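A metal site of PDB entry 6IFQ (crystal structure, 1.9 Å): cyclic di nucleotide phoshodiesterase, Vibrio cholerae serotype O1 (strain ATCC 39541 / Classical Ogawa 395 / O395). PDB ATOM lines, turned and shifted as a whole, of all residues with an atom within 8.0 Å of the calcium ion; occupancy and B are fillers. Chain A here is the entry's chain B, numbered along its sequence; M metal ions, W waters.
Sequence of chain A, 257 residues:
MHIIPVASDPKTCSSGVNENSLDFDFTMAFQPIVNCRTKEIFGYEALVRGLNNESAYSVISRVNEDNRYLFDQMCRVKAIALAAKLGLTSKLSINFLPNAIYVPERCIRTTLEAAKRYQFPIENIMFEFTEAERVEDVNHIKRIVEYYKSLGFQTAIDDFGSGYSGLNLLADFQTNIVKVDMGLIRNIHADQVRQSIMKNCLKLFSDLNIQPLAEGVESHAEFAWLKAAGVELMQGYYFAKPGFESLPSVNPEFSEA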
ATOM      1  N   GLU A  45       9.017 -19.337  24.268  1.00  0.00           N
ATOM      2  CA  GLU A  45       7.803 -18.690  23.818  1.00  0.00           C
ATOM      3  C   GLU A  45       6.613 -19.411  24.406  1.00  0.00           C
ATOM      4  O   GLU A  45       6.541 -20.637  24.374  1.00  0.00           O
ATOM      5  CB  GLU A  45       7.698 -18.677  22.277  1.00  0.00           C
ATOM      6  CG  GLU A  45       6.476 -17.940  21.769  1.00  0.00           C
ATOM      7  CD  GLU A  45       6.362 -17.900  20.245  1.00  0.00           C
ATOM      8  OE1 GLU A  45       7.290 -18.365  19.552  1.00  0.00           O
ATOM      9  OE2 GLU A  45       5.334 -17.405  19.737  1.00  0.00           O
ATOM     10  N   ALA A  46       5.673 -18.650  24.949  1.00  0.00           N
ATOM     11  CA  ALA A  46       4.374 -19.196  25.347  1.00  0.00           C
ATOM     12  C   ALA A  46       3.429 -19.304  24.130  1.00  0.00           C
ATOM     13  O   ALA A  46       3.165 -18.313  23.461  1.00  0.00           O
ATOM     14  CB  ALA A  46       3.743 -18.357  26.419  1.00  0.00           C
ATOM     15  N   LEU A  47       2.914 -20.507  23.907  1.00  0.00           N
ATOM     16  CA  LEU A  47       2.015 -20.812  22.796  1.00  0.00           C
ATOM     17  C   LEU A  47       0.667 -21.333  23.279  1.00  0.00           C
ATOM     18  O   LEU A  47       0.617 -22.306  24.030  1.00  0.00           O
ATOM     19  CB  LEU A  47       2.654 -21.833  21.860  1.00  0.00           C
ATOM     20  CG  LEU A  47       3.928 -21.363  21.158  1.00  0.00           C
ATOM     21  CD1 LEU A  47       4.724 -22.569  20.680  1.00  0.00           C
ATOM     22  CD2 LEU A  47       3.546 -20.425  20.010  1.00  0.00           C
ATOM     23  N   SER A  93       8.546 -15.344  26.490  1.00  0.00           N
ATOM     24  CA  SER A  93       8.140 -14.573  25.301  1.00  0.00           C
ATOM     25  C   SER A  93       6.677 -14.820  24.962  1.00  0.00           C
ATOM     26  O   SER A  93       6.230 -15.967  24.867  1.00  0.00           O
ATOM     27  CB  SER A  93       9.021 -14.910  24.102  1.00  0.00           C
ATOM     28  OG  SER A  93       8.801 -13.970  23.068  1.00  0.00           O
ATOM     29  N   ILE A  94       5.932 -13.733  24.797  1.00  0.00           N
ATOM     30  CA  ILE A  94       4.487 -13.816  24.642  1.00  0.00           C
ATOM     31  C   ILE A  94       4.032 -13.059  23.399  1.00  0.00           C
ATOM     32  O   ILE A  94       4.454 -11.923  23.168  1.00  0.00           O
ATOM     33  CB  ILE A  94       3.768 -13.244  25.897  1.00  0.00           C
ATOM     34  CG1 ILE A  94       4.339 -13.876  27.168  1.00  0.00           C
ATOM     35  CG2 ILE A  94       2.276 -13.482  25.811  1.00  0.00           C
ATOM     36  CD1 ILE A  94       3.522 -13.585  28.421  1.00  0.00           C
ATOM     37  N   ASN A  95       3.195 -13.703  22.597  1.00  0.00           N
ATOM     38  CA  ASN A  95       2.630 -13.065  21.418  1.00  0.00           C
ATOM     39  C   ASN A  95       1.641 -11.975  21.782  1.00  0.00           C
ATOM     40  O   ASN A  95       0.693 -12.211  22.540  1.00  0.00           O
ATOM     41  CB  ASN A  95       1.935 -14.093  20.535  1.00  0.00           C
ATOM     42  CG  ASN A  95       2.859 -15.185  20.090  1.00  0.00           C
ATOM     43  OD1 ASN A  95       3.493 -15.074  19.043  1.00  0.00           O
ATOM     44  ND2 ASN A  95       2.947 -16.248  20.885  1.00  0.00           N
ATOM     45  N   PHE A  96       1.848 -10.799  21.217  1.00  0.00           N
ATOM     46  CA  PHE A  96       0.923  -9.683  21.377  1.00  0.00           C
ATOM     47  C   PHE A  96      -0.104  -9.738  20.244  1.00  0.00           C
ATOM     48  O   PHE A  96       0.261  -9.733  19.057  1.00  0.00           O
ATOM     49  CB  PHE A  96       1.684  -8.359  21.377  1.00  0.00           C
ATOM     50  CG  PHE A  96       0.807  -7.145  21.512  1.00  0.00           C
ATOM     51  CD1 PHE A  96       0.313  -6.502  20.393  1.00  0.00           C
ATOM     52  CD2 PHE A  96       0.491  -6.641  22.764  1.00  0.00           C
ATOM     53  CE1 PHE A  96      -0.495  -5.384  20.521  1.00  0.00           C
ATOM     54  CE2 PHE A  96      -0.317  -5.523  22.893  1.00  0.00           C
ATOM     55  CZ  PHE A  96      -0.809  -4.891  21.782  1.00  0.00           C
ATOM     56  N   PHE A 127       7.501  -9.303  24.494  1.00  0.00           N
ATOM     57  CA  PHE A 127       6.282  -9.374  23.713  1.00  0.00           C
ATOM     58  C   PHE A 127       6.627  -9.384  22.230  1.00  0.00           C
ATOM     59  O   PHE A 127       7.481  -8.624  21.781  1.00  0.00           O
ATOM     60  CB  PHE A 127       5.343  -8.215  24.047  1.00  0.00           C
ATOM     61  CG  PHE A 127       4.560  -8.419  25.303  1.00  0.00           C
ATOM     62  CD1 PHE A 127       3.403  -9.178  25.305  1.00  0.00           C
ATOM     63  CD2 PHE A 127       4.973  -7.852  26.501  1.00  0.00           C
ATOM     64  CE1 PHE A 127       2.677  -9.375  26.480  1.00  0.00           C
ATOM     65  CE2 PHE A 127       4.255  -8.039  27.676  1.00  0.00           C
ATOM     66  CZ  PHE A 127       3.116  -8.803  27.653  1.00  0.00           C
ATOM     67  N   GLU A 128       5.983 -10.269  21.481  1.00  0.00           N
ATOM     68  CA  GLU A 128       6.242 -10.456  20.059  1.00  0.00           C
ATOM     69  C   GLU A 128       5.168  -9.766  19.260  1.00  0.00           C
ATOM     70  O   GLU A 128       3.989 -10.055  19.427  1.00  0.00           O
ATOM     71  CB  GLU A 128       6.312 -11.949  19.715  1.00  0.00           C
ATOM     72  CG  GLU A 128       7.253 -12.727  20.639  1.00  0.00           C
ATOM     73  CD  GLU A 128       7.595 -14.102  20.097  1.00  0.00           C
ATOM     74  OE1 GLU A 128       8.407 -14.812  20.726  1.00  0.00           O
ATOM     75  OE2 GLU A 128       7.064 -14.454  19.035  1.00  0.00           O
ATOM     76  N   PHE A 129       5.568  -8.826  18.398  1.00  0.00           N
ATOM     77  CA  PHE A 129       4.593  -8.062  17.622  1.00  0.00           C
ATOM     78  C   PHE A 129       4.480  -8.583  16.180  1.00  0.00           C
ATOM     79  O   PHE A 129       5.468  -8.641  15.443  1.00  0.00           O
ATOM     80  CB  PHE A 129       4.962  -6.579  17.616  1.00  0.00           C
ATOM     81  CG  PHE A 129       4.990  -5.940  18.978  1.00  0.00           C
ATOM     82  CD1 PHE A 129       6.148  -5.928  19.730  1.00  0.00           C
ATOM     83  CD2 PHE A 129       3.847  -5.340  19.504  1.00  0.00           C
ATOM     84  CE1 PHE A 129       6.181  -5.341  20.981  1.00  0.00           C
ATOM     85  CE2 PHE A 129       3.868  -4.743  20.748  1.00  0.00           C
ATOM     86  CZ  PHE A 129       5.037  -4.750  21.496  1.00  0.00           C
ATOM     87  N   THR A 130       3.262  -8.939  15.789  1.00  0.00           N
ATOM     88  CA  THR A 130       3.035  -9.472  14.449  1.00  0.00           C
ATOM     89  C   THR A 130       1.853  -8.799  13.780  1.00  0.00           C
ATOM     90  O   THR A 130       1.000  -8.214  14.445  1.00  0.00           O
ATOM     91  CB  THR A 130       2.778 -10.995  14.490  1.00  0.00           C
ATOM     92  OG1 THR A 130       2.278 -11.413  13.217  1.00  0.00           O
ATOM     93  CG2 THR A 130       1.749 -11.325  15.558  1.00  0.00           C
ATOM     94  N   ALA A 156       9.811  -7.803  20.409  1.00  0.00           N
ATOM     95  CA  ALA A 156      10.252  -8.443  19.165  1.00  0.00           C
ATOM     96  C   ALA A 156       9.266  -8.226  18.055  1.00  0.00           C
ATOM     97  O   ALA A 156       8.060  -8.192  18.284  1.00  0.00           O
ATOM     98  CB  ALA A 156      10.471  -9.936  19.390  1.00  0.00           C
ATOM     99  N   ILE A 157       9.787  -8.085  16.838  1.00  0.00           N
ATOM    100  CA  ILE A 157       8.949  -8.266  15.673  1.00  0.00           C
ATOM    101  C   ILE A 157       8.968  -9.735  15.280  1.00  0.00           C
ATOM    102  O   ILE A 157      10.017 -10.351  15.149  1.00  0.00           O
ATOM    103  CB  ILE A 157       9.413  -7.395  14.501  1.00  0.00           C
ATOM    104  CG1 ILE A 157       9.083  -5.940  14.795  1.00  0.00           C
ATOM    105  CG2 ILE A 157       8.690  -7.827  13.226  1.00  0.00           C
ATOM    106  CD1 ILE A 157      10.155  -4.994  14.343  1.00  0.00           C
ATOM    107  N   ASP A 158       7.774 -10.287  15.113  1.00  0.00           N
ATOM    108  CA  ASP A 158       7.605 -11.686  14.786  1.00  0.00           C
ATOM    109  C   ASP A 158       7.402 -11.896  13.272  1.00  0.00           C
ATOM    110  O   ASP A 158       6.975 -10.978  12.561  1.00  0.00           O
ATOM    111  CB  ASP A 158       6.414 -12.254  15.562  1.00  0.00           C
ATOM    112  CG  ASP A 158       6.480 -13.745  15.722  1.00  0.00           C
ATOM    113  OD1 ASP A 158       7.570 -14.314  15.498  1.00  0.00           O
ATOM    114  OD2 ASP A 158       5.451 -14.367  16.059  1.00  0.00           O
ATOM    115  N   ASP A 159       7.713 -13.113  12.811  1.00  0.00           N
ATOM    116  CA  ASP A 159       7.437 -13.520  11.426  1.00  0.00           C
ATOM    117  C   ASP A 159       7.944 -12.516  10.389  1.00  0.00           C
ATOM    118  O   ASP A 159       7.308 -12.309   9.346  1.00  0.00           O
ATOM    119  CB  ASP A 159       5.933 -13.730  11.223  1.00  0.00           C
ATOM    120  CG  ASP A 159       5.368 -14.827  12.113  1.00  0.00           C
ATOM    121  OD1 ASP A 159       6.136 -15.735  12.506  1.00  0.00           O
ATOM    122  OD2 ASP A 159       4.154 -14.785  12.417  1.00  0.00           O
ATOM    123  N   LYS A 179      12.431 -11.724  14.931  1.00  0.00           N
ATOM    124  CA  LYS A 179      12.314 -13.130  14.604  1.00  0.00           C
ATOM    125  C   LYS A 179      12.027 -13.296  13.102  1.00  0.00           C
ATOM    126  O   LYS A 179      10.959 -12.962  12.630  1.00  0.00           O
ATOM    127  CB  LYS A 179      11.211 -13.802  15.430  1.00  0.00           C
ATOM    128  CG  LYS A 179      11.286 -13.425  16.931  1.00  0.00           C
ATOM    129  CD  LYS A 179      10.191 -14.123  17.731  1.00  0.00           C
ATOM    130  CE  LYS A 179      10.530 -15.597  17.946  1.00  0.00           C
ATOM    131  NZ  LYS A 179       9.424 -16.390  18.570  1.00  0.00           N
ATOM    132  N   GLU A 215      13.522 -18.564  13.381  1.00  0.00           N
ATOM    133  CA  GLU A 215      12.551 -19.561  13.806  1.00  0.00           C
ATOM    134  C   GLU A 215      12.326 -20.624  12.737  1.00  0.00           C
ATOM    135  O   GLU A 215      12.781 -20.481  11.615  1.00  0.00           O
ATOM    136  CB  GLU A 215      11.214 -18.927  14.168  1.00  0.00           C
ATOM    137  CG  GLU A 215      11.030 -17.496  13.764  1.00  0.00           C
ATOM    138  CD  GLU A 215       9.651 -16.984  14.115  1.00  0.00           C
ATOM    139  OE1 GLU A 215       9.139 -17.358  15.204  1.00  0.00           O
ATOM    140  OE2 GLU A 215       9.068 -16.223  13.307  1.00  0.00           O
ATOM    141  N   GLN A 235      15.035 -20.972  17.146  1.00  0.00           N
ATOM    142  CA  GLN A 235      13.871 -21.660  17.663  1.00  0.00           C
ATOM    143  C   GLN A 235      13.397 -22.648  16.610  1.00  0.00           C
ATOM    144  O   GLN A 235      13.449 -22.346  15.411  1.00  0.00           O
ATOM    145  CB  GLN A 235      12.763 -20.664  18.004  1.00  0.00           C
ATOM    146  CG  GLN A 235      11.462 -21.272  18.475  1.00  0.00           C
ATOM    147  CD  GLN A 235      10.487 -20.211  18.966  1.00  0.00           C
ATOM    148  OE1 GLN A 235      10.756 -19.016  18.885  1.00  0.00           O
ATOM    149  NE2 GLN A 235       9.353 -20.646  19.493  1.00  0.00           N
HETATM  150 CA    CA M   1       5.400 -15.676  18.046  1.00  0.00          CA
HETATM  151  O   HOH W   1       7.134 -16.826  17.186  1.00  0.00           O
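Four residues have an atom within 4 Å of the calcium ion: Glu 45, Asn 95, Glu 128 and Asp 158.
The nearest printed residue that does not touch the calcium ion is Lys 179 (4.1 Å).
The calcium ion is bound by OD1 of Asn 95, 2.2 Å away.
The calcium ion is bound by water W1, 2.3 Å away.
The calcium ion is bound by the side-chain carboxylate (OE2) of Glu 128, 2.3 Å away.
The calcium ion is bound by OD2 of Asp 158 (2.4 Å).
OE2 of Glu 45 binds the calcium ion (2.4 Å).
The calcium ion has five donor atoms within binding distance.
The side-chain amino group (NZ) of Lys 179 lies within salt-bridge range of the side-chain carboxylate (OE1) of Glu 128, at 2.9 Å.
The side-chain carboxylate of Glu 45 is in hydrogen-bond range of the side-chain amide nitrogen of Gln 235 (3.1 Å).
The side-chain amino group (NZ) of Lys 179 lies within salt-bridge range of the side-chain carboxylate (OE1) of Glu 45.
The side-chain hydroxyl (OG) of Ser 93 sits at hydrogen-bond distance from the side-chain carboxylate (OE1) of Glu 128.
The backbone carbonyl oxygen (O) of Phe 129 lies within hydrogen-bond range of the backbone NH (N) of Asp 158.
N of Glu 128 is in hydrogen-bond range of O of Ile 94 (2.8 Å).
O of Glu 128 sits at hydrogen-bond distance from N of Phe 96, 2.9 Å away.
The side-chain amide nitrogen (ND2) of Asn 95 lies within hydrogen-bond range of the backbone carbonyl oxygen (O) of Ala 46 (3.3 Å).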
